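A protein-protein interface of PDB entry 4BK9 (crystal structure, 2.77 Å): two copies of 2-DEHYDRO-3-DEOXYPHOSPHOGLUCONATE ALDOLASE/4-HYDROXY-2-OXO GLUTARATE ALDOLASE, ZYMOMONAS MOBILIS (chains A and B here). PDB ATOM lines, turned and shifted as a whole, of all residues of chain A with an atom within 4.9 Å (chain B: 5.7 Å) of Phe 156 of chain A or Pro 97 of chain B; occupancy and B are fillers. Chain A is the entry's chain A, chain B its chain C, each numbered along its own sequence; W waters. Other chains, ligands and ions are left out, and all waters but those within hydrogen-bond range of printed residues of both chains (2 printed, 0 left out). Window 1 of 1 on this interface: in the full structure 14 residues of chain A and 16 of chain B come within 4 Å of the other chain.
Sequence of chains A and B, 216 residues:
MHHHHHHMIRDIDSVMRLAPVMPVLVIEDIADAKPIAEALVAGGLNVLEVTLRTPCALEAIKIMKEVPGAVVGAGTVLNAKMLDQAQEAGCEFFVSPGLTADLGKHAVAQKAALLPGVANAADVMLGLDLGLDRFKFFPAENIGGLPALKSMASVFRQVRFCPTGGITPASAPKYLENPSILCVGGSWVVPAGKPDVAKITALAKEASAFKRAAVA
N of Gly 98 of chain B is in hydrogen-bond range of SD of Met 125 of chain A (3.4 Å).
The side-chain hydroxyl (OG) of Ser 96 of chain B is in hydrogen-bond range of the backbone carbonyl oxygen (O) of Gly 98 of chain B (2.6 Å). The backbone carbonyl oxygen (O) of Val 118 of chain B is in hydrogen-bond range of the backbone NH (N) of Phe 138 of chain B, at 3.1 Å. The backbone carbonyl oxygen (O) of Val 95 of chain B is in hydrogen-bond range of the backbone NH (N) of Thr 76 of chain B.
Water W2 bridges O of Leu 78 of chain B (2.6 Å) and O of Met 125 of chain A (3.3 Å). Water W1 bridges N of Ala 121 of chain A (2.8 Å) and O of Phe 138 of chain B (3.1 Å).
Pro 97 of chain B touches Ala 121 of chain A. Gly 98 of chain B touches Ala 121 of chain A (N to CB, 3.9 Å). CE of Met 125 of chain A touches O of Leu 78 of chain B, at 3.4 Å. Leu 128 of chain A touches Leu 78 of chain B (CD1 to CD1, 3.8 Å). Thr 76 of chain B touches Val 155 of chain A (CG2 to O, 3.4 Å). Pro 97 of chain B touches Val 155 of chain A (CG to CG1, 3.7 Å). Val 155 of chain A touches Phe 138 of chain B. Phe 156 of chain A touches Leu 78 of chain B. Pro 97 of chain B touches Phe 156 of chain A. Leu 78 of chain B touches Gln 158 of chain A.
Printed residues of chain B within 4 Å of Ala 121 of chain A: Pro 97 (3.4 Å) and Gly 98 (3.9 Å). Of the printed residues of chain B, Leu 128 of chain A touches Leu 78 (3.8 Å). Ala 153 of chain A touches none of the printed residues of chain B. Printed residues of chain B within 4 Å of Val 155 of chain A: Thr 76, Pro 97 and Phe 138. Of chain B, only Leu 78 and Pro 97 come within 4 Å of Phe 156 of chain A. Of the printed residues of chain B, Gln 158 of chain A touches Leu 78. Printed residues of chain A within 4 Å of Thr 76 of chain B: Val 155 (3.4 Å). Of the printed residues of chain A, Pro 97 of chain B touches Ala 121 (3.4 Å), Val 155 (3.7 Å) and Phe 156 (3.9 Å). Pro 116 of chain B touches none of the printed residues of chain A. The nearest residue of chain B that does not touch Phe 156 of chain A is Thr 76 of chain B (5.5 Å).
Hydrophobic or aromatic side chains of chain B that line the printed part of chain A: Leu 78, Pro 97 and Phe 138. Hydrophobic or aromatic side chains of chain A within 4 Å of the printed part of chain B: Ala 121, Met 125, Leu 128, Val 155 and Phe 156. Among the printed residues, 11 pairs touch across the chains. Among the printed residues, no Asp or Glu carboxylate lies within 4 Å of a Lys or Arg side-chain nitrogen of the other chain.
No position is printed for both chains. Of the 11 pairs that touch across the chains among the printed residues, none has its exchanged pair printed and touching as well.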
ATOM      1  N   ALA A 121      -4.812  -9.560 -21.668  1.00  0.00           N
ATOM      2  CA  ALA A 121      -6.219  -9.309 -21.959  1.00  0.00           C
ATOM      3  C   ALA A 121      -6.441  -8.130 -22.900  1.00  0.00           C
ATOM      4  O   ALA A 121      -7.341  -8.125 -23.678  1.00  0.00           O
ATOM      5  CB  ALA A 121      -6.975  -9.076 -20.671  1.00  0.00           C
ATOM      6  N   VAL A 124      -6.175  -9.353 -26.413  1.00  0.00           N
ATOM      7  CA  VAL A 124      -7.341 -10.105 -26.834  1.00  0.00           C
ATOM      8  C   VAL A 124      -8.495  -9.134 -27.084  1.00  0.00           C
ATOM      9  O   VAL A 124      -9.228  -9.259 -28.046  1.00  0.00           O
ATOM     10  CB  VAL A 124      -7.770 -11.143 -25.756  1.00  0.00           C
ATOM     11  CG1 VAL A 124      -9.079 -11.816 -26.122  1.00  0.00           C
ATOM     12  CG2 VAL A 124      -6.669 -12.176 -25.556  1.00  0.00           C
ATOM     13  N   MET A 125      -8.666  -8.172 -26.196  1.00  0.00           N
ATOM     14  CA  MET A 125      -9.768  -7.253 -26.314  1.00  0.00           C
ATOM     15  C   MET A 125      -9.705  -6.440 -27.600  1.00  0.00           C
ATOM     16  O   MET A 125     -10.725  -6.157 -28.215  1.00  0.00           O
ATOM     17  CB  MET A 125      -9.804  -6.363 -25.092  1.00  0.00           C
ATOM     18  CG  MET A 125     -10.412  -7.082 -23.914  1.00  0.00           C
ATOM     19  SD  MET A 125     -10.286  -6.154 -22.455  1.00  0.00           S
ATOM     20  CE  MET A 125     -11.481  -4.863 -22.709  1.00  0.00           C
ATOM     21  N   LEU A 128     -10.814  -8.773 -30.311  1.00  0.00           N
ATOM     22  CA  LEU A 128     -12.278  -8.923 -30.309  1.00  0.00           C
ATOM     23  C   LEU A 128     -12.911  -7.723 -30.948  1.00  0.00           C
ATOM     24  O   LEU A 128     -13.797  -7.875 -31.717  1.00  0.00           O
ATOM     25  CB  LEU A 128     -12.819  -9.139 -28.891  1.00  0.00           C
ATOM     26  CG  LEU A 128     -12.476 -10.481 -28.253  1.00  0.00           C
ATOM     27  CD1 LEU A 128     -12.750 -10.468 -26.750  1.00  0.00           C
ATOM     28  CD2 LEU A 128     -13.253 -11.580 -28.939  1.00  0.00           C
ATOM     29  N   MET A 152      -6.982 -16.725 -18.988  1.00  0.00           N
ATOM     30  CA  MET A 152      -7.530 -15.955 -20.114  1.00  0.00           C
ATOM     31  C   MET A 152      -8.741 -16.646 -20.674  1.00  0.00           C
ATOM     32  O   MET A 152      -9.700 -16.026 -21.036  1.00  0.00           O
ATOM     33  CB  MET A 152      -6.579 -15.900 -21.295  1.00  0.00           C
ATOM     34  CG  MET A 152      -5.168 -15.446 -21.042  1.00  0.00           C
ATOM     35  SD  MET A 152      -4.893 -13.842 -21.784  1.00  0.00           S
ATOM     36  CE  MET A 152      -5.535 -12.979 -20.336  1.00  0.00           C
ATOM     37  N   ALA A 153      -8.633 -17.950 -20.837  1.00  0.00           N
ATOM     38  CA  ALA A 153      -9.671 -18.752 -21.437  1.00  0.00           C
ATOM     39  C   ALA A 153     -10.935 -18.741 -20.628  1.00  0.00           C
ATOM     40  O   ALA A 153     -12.016 -18.749 -21.182  1.00  0.00           O
ATOM     41  CB  ALA A 153      -9.207 -20.166 -21.554  1.00  0.00           C
ATOM     42  N   SER A 154     -10.825 -18.637 -19.324  1.00  0.00           N
ATOM     43  CA  SER A 154     -12.018 -18.685 -18.543  1.00  0.00           C
ATOM     44  C   SER A 154     -12.697 -17.310 -18.555  1.00  0.00           C
ATOM     45  O   SER A 154     -13.913 -17.213 -18.282  1.00  0.00           O
ATOM     46  CB  SER A 154     -11.727 -19.249 -17.145  1.00  0.00           C
ATOM     47  OG  SER A 154     -11.307 -18.241 -16.276  1.00  0.00           O
ATOM     48  N   VAL A 155     -11.926 -16.257 -18.866  1.00  0.00           N
ATOM     49  CA  VAL A 155     -12.486 -14.912 -18.993  1.00  0.00           C
ATOM     50  C   VAL A 155     -13.116 -14.677 -20.367  1.00  0.00           C
ATOM     51  O   VAL A 155     -14.172 -14.068 -20.465  1.00  0.00           O
ATOM     52  CB  VAL A 155     -11.427 -13.821 -18.696  1.00  0.00           C
ATOM     53  CG1 VAL A 155     -11.868 -12.467 -19.234  1.00  0.00           C
ATOM     54  CG2 VAL A 155     -11.185 -13.719 -17.199  1.00  0.00           C
ATOM     55  N   PHE A 156     -12.435 -15.112 -21.418  1.00  0.00           N
ATOM     56  CA  PHE A 156     -12.854 -14.893 -22.788  1.00  0.00           C
ATOM     57  C   PHE A 156     -13.334 -16.230 -23.279  1.00  0.00           C
ATOM     58  O   PHE A 156     -12.578 -17.005 -23.880  1.00  0.00           O
ATOM     59  CB  PHE A 156     -11.672 -14.419 -23.654  1.00  0.00           C
ATOM     60  CG  PHE A 156     -11.052 -13.165 -23.202  1.00  0.00           C
ATOM     61  CD1 PHE A 156     -11.705 -11.952 -23.414  1.00  0.00           C
ATOM     62  CD2 PHE A 156      -9.796 -13.176 -22.632  1.00  0.00           C
ATOM     63  CE1 PHE A 156     -11.130 -10.780 -23.026  1.00  0.00           C
ATOM     64  CE2 PHE A 156      -9.229 -12.000 -22.212  1.00  0.00           C
ATOM     65  CZ  PHE A 156      -9.898 -10.803 -22.407  1.00  0.00           C
ATOM     66  N   ARG A 157     -14.593 -16.481 -23.023  1.00  0.00           N
ATOM     67  CA  ARG A 157     -15.161 -17.795 -23.201  1.00  0.00           C
ATOM     68  C   ARG A 157     -15.376 -18.067 -24.657  1.00  0.00           C
ATOM     69  O   ARG A 157     -15.326 -19.221 -25.075  1.00  0.00           O
ATOM     70  CB  ARG A 157     -16.498 -17.910 -22.457  1.00  0.00           C
ATOM     71  CG  ARG A 157     -16.396 -17.596 -20.960  1.00  0.00           C
ATOM     72  CD  ARG A 157     -16.070 -18.809 -20.077  1.00  0.00           C
ATOM     73  NE  ARG A 157     -17.273 -19.232 -19.356  1.00  0.00           N
ATOM     74  CZ  ARG A 157     -17.384 -19.321 -18.044  1.00  0.00           C
ATOM     75  NH1 ARG A 157     -16.351 -19.065 -17.246  1.00  0.00           N
ATOM     76  NH2 ARG A 157     -18.548 -19.684 -17.521  1.00  0.00           N
ATOM     77  N   GLN A 158     -15.557 -17.012 -25.452  1.00  0.00           N
ATOM     78  CA  GLN A 158     -15.838 -17.157 -26.893  1.00  0.00           C
ATOM     79  C   GLN A 158     -14.554 -17.362 -27.741  1.00  0.00           C
ATOM     80  O   GLN A 158     -14.626 -17.633 -28.896  1.00  0.00           O
ATOM     81  CB  GLN A 158     -16.709 -15.985 -27.410  1.00  0.00           C
ATOM     82  CG  GLN A 158     -15.990 -14.628 -27.563  1.00  0.00           C
ATOM     83  CD  GLN A 158     -15.841 -13.756 -26.256  1.00  0.00           C
ATOM     84  OE1 GLN A 158     -15.147 -14.128 -25.250  1.00  0.00           O
ATOM     85  NE2 GLN A 158     -16.469 -12.553 -26.295  1.00  0.00           N
ATOM     86  N   VAL A 159     -13.394 -17.250 -27.126  1.00  0.00           N
ATOM     87  CA  VAL A 159     -12.134 -17.208 -27.792  1.00  0.00           C
ATOM     88  C   VAL A 159     -11.431 -18.570 -27.717  1.00  0.00           C
ATOM     89  O   VAL A 159     -11.572 -19.313 -26.757  1.00  0.00           O
ATOM     90  CB  VAL A 159     -11.298 -16.102 -27.111  1.00  0.00           C
ATOM     91  CG1 VAL A 159      -9.829 -16.235 -27.433  1.00  0.00           C
ATOM     92  CG2 VAL A 159     -11.760 -14.727 -27.548  1.00  0.00           C
ATOM     93  N   THR B  76     -16.068  -8.387 -16.703  1.00  0.00           N
ATOM     94  CA  THR B  76     -15.858  -8.993 -17.998  1.00  0.00           C
ATOM     95  C   THR B  76     -16.591  -8.184 -19.040  1.00  0.00           C
ATOM     96  O   THR B  76     -17.193  -8.723 -20.018  1.00  0.00           O
ATOM     97  CB  THR B  76     -16.254 -10.469 -18.042  1.00  0.00           C
ATOM     98  OG1 THR B  76     -15.918 -11.066 -16.800  1.00  0.00           O
ATOM     99  CG2 THR B  76     -15.500 -11.179 -19.150  1.00  0.00           C
ATOM    100  N   VAL B  77     -16.466  -6.873 -18.838  1.00  0.00           N
ATOM    101  CA  VAL B  77     -16.994  -5.913 -19.755  1.00  0.00           C
ATOM    102  C   VAL B  77     -15.966  -5.680 -20.837  1.00  0.00           C
ATOM    103  O   VAL B  77     -14.937  -5.111 -20.567  1.00  0.00           O
ATOM    104  CB  VAL B  77     -17.308  -4.609 -19.029  1.00  0.00           C
ATOM    105  CG1 VAL B  77     -17.757  -3.555 -20.035  1.00  0.00           C
ATOM    106  CG2 VAL B  77     -18.412  -4.849 -18.005  1.00  0.00           C
ATOM    107  N   LEU B  78     -16.207  -6.197 -22.029  1.00  0.00           N
ATOM    108  CA  LEU B  78     -15.177  -6.210 -23.064  1.00  0.00           C
ATOM    109  C   LEU B  78     -15.254  -5.007 -23.965  1.00  0.00           C
ATOM    110  O   LEU B  78     -14.299  -4.695 -24.680  1.00  0.00           O
ATOM    111  CB  LEU B  78     -15.281  -7.482 -23.918  1.00  0.00           C
ATOM    112  CG  LEU B  78     -15.264  -8.785 -23.108  1.00  0.00           C
ATOM    113  CD1 LEU B  78     -15.324  -9.997 -24.042  1.00  0.00           C
ATOM    114  CD2 LEU B  78     -14.059  -8.832 -22.179  1.00  0.00           C
ATOM    115  N   VAL B  95     -16.086  -3.643 -14.373  1.00  0.00           N
ATOM    116  CA  VAL B  95     -14.730  -4.147 -14.364  1.00  0.00           C
ATOM    117  C   VAL B  95     -14.481  -4.787 -15.711  1.00  0.00           C
ATOM    118  O   VAL B  95     -15.371  -5.440 -16.264  1.00  0.00           O
ATOM    119  CB  VAL B  95     -14.515  -5.162 -13.228  1.00  0.00           C
ATOM    120  CG1 VAL B  95     -13.073  -5.617 -13.199  1.00  0.00           C
ATOM    121  CG2 VAL B  95     -14.900  -4.567 -11.882  1.00  0.00           C
ATOM    122  N   SER B  96     -13.278  -4.588 -16.239  1.00  0.00           N
ATOM    123  CA  SER B  96     -12.868  -5.266 -17.447  1.00  0.00           C
ATOM    124  C   SER B  96     -11.518  -5.909 -17.230  1.00  0.00           C
ATOM    125  O   SER B  96     -10.735  -5.461 -16.437  1.00  0.00           O
ATOM    126  CB  SER B  96     -12.859  -4.290 -18.603  1.00  0.00           C
ATOM    127  OG  SER B  96     -11.846  -3.325 -18.419  1.00  0.00           O
ATOM    128  N   PRO B  97     -11.257  -6.993 -17.944  1.00  0.00           N
ATOM    129  CA  PRO B  97      -9.980  -7.698 -17.792  1.00  0.00           C
ATOM    130  C   PRO B  97      -8.790  -6.934 -18.350  1.00  0.00           C
ATOM    131  O   PRO B  97      -7.654  -7.154 -17.953  1.00  0.00           O
ATOM    132  CB  PRO B  97     -10.197  -9.029 -18.551  1.00  0.00           C
ATOM    133  CG  PRO B  97     -11.370  -8.794 -19.455  1.00  0.00           C
ATOM    134  CD  PRO B  97     -12.080  -7.540 -19.047  1.00  0.00           C
ATOM    135  N   GLY B  98      -9.054  -6.103 -19.331  1.00  0.00           N
ATOM    136  CA  GLY B  98      -8.047  -5.262 -19.918  1.00  0.00           C
ATOM    137  C   GLY B  98      -8.662  -3.911 -20.279  1.00  0.00           C
ATOM    138  O   GLY B  98      -9.834  -3.669 -20.043  1.00  0.00           O
ATOM    139  N   LEU B  99      -7.864  -3.061 -20.920  1.00  0.00           N
ATOM    140  CA  LEU B  99      -8.330  -1.748 -21.307  1.00  0.00           C
ATOM    141  C   LEU B  99      -8.127  -1.494 -22.791  1.00  0.00           C
ATOM    142  O   LEU B  99      -7.090  -1.750 -23.294  1.00  0.00           O
ATOM    143  CB  LEU B  99      -7.574  -0.717 -20.481  1.00  0.00           C
ATOM    144  CG  LEU B  99      -7.913   0.731 -20.720  1.00  0.00           C
ATOM    145  CD1 LEU B  99      -9.367   1.058 -20.407  1.00  0.00           C
ATOM    146  CD2 LEU B  99      -6.984   1.551 -19.868  1.00  0.00           C
ATOM    147  N   PRO B 116     -10.579  -0.818 -14.980  1.00  0.00           N
ATOM    148  CA  PRO B 116     -10.093  -1.708 -16.018  1.00  0.00           C
ATOM    149  C   PRO B 116      -8.836  -2.478 -15.657  1.00  0.00           C
ATOM    150  O   PRO B 116      -8.009  -2.023 -14.894  1.00  0.00           O
ATOM    151  CB  PRO B 116      -9.781  -0.757 -17.157  1.00  0.00           C
ATOM    152  CG  PRO B 116      -9.471   0.565 -16.486  1.00  0.00           C
ATOM    153  CD  PRO B 116     -10.018   0.529 -15.100  1.00  0.00           C
ATOM    154  N   GLY B 117      -8.678  -3.621 -16.299  1.00  0.00           N
ATOM    155  CA  GLY B 117      -7.505  -4.462 -16.131  1.00  0.00           C
ATOM    156  C   GLY B 117      -6.267  -3.905 -16.803  1.00  0.00           C
ATOM    157  O   GLY B 117      -6.311  -3.376 -17.929  1.00  0.00           O
ATOM    158  N   VAL B 118      -5.160  -4.008 -16.088  1.00  0.00           N
ATOM    159  CA  VAL B 118      -3.844  -3.744 -16.652  1.00  0.00           C
ATOM    160  C   VAL B 118      -2.905  -4.915 -16.423  1.00  0.00           C
ATOM    161  O   VAL B 118      -3.061  -5.655 -15.468  1.00  0.00           O
ATOM    162  CB  VAL B 118      -3.217  -2.437 -16.119  1.00  0.00           C
ATOM    163  CG1 VAL B 118      -4.108  -1.258 -16.492  1.00  0.00           C
ATOM    164  CG2 VAL B 118      -2.963  -2.504 -14.609  1.00  0.00           C
ATOM    165  N   LYS B 136      -7.228  -2.647 -12.204  1.00  0.00           N
ATOM    166  CA  LYS B 136      -7.281  -4.026 -11.774  1.00  0.00           C
ATOM    167  C   LYS B 136      -6.030  -4.649 -12.362  1.00  0.00           C
ATOM    168  O   LYS B 136      -5.722  -4.420 -13.482  1.00  0.00           O
ATOM    169  CB  LYS B 136      -8.492  -4.655 -12.442  1.00  0.00           C
ATOM    170  CG  LYS B 136      -8.677  -6.170 -12.398  1.00  0.00           C
ATOM    171  CD  LYS B 136      -9.936  -6.536 -11.619  1.00  0.00           C
ATOM    172  CE  LYS B 136      -9.782  -6.117 -10.114  1.00  0.00           C
ATOM    173  NZ  LYS B 136     -10.964  -6.235  -9.168  1.00  0.00           N
ATOM    174  N   PHE B 138      -4.350  -7.807 -13.588  1.00  0.00           N
ATOM    175  CA  PHE B 138      -5.005  -9.052 -13.923  1.00  0.00           C
ATOM    176  C   PHE B 138      -4.346  -9.737 -15.074  1.00  0.00           C
ATOM    177  O   PHE B 138      -3.911  -9.067 -15.988  1.00  0.00           O
ATOM    178  CB  PHE B 138      -6.461  -8.763 -14.336  1.00  0.00           C
ATOM    179  CG  PHE B 138      -7.164  -9.953 -14.899  1.00  0.00           C
ATOM    180  CD1 PHE B 138      -7.686 -10.899 -14.068  1.00  0.00           C
ATOM    181  CD2 PHE B 138      -7.244 -10.146 -16.261  1.00  0.00           C
ATOM    182  CE1 PHE B 138      -8.257 -12.035 -14.574  1.00  0.00           C
ATOM    183  CE2 PHE B 138      -7.819 -11.267 -16.779  1.00  0.00           C
ATOM    184  CZ  PHE B 138      -8.318 -12.218 -15.929  1.00  0.00           C
HETATM  185  O   HOH W   1      -3.792  -9.870 -19.031  1.00  0.00           O
HETATM  186  O   HOH W   2     -13.505  -6.345 -26.485  1.00  0.00           O
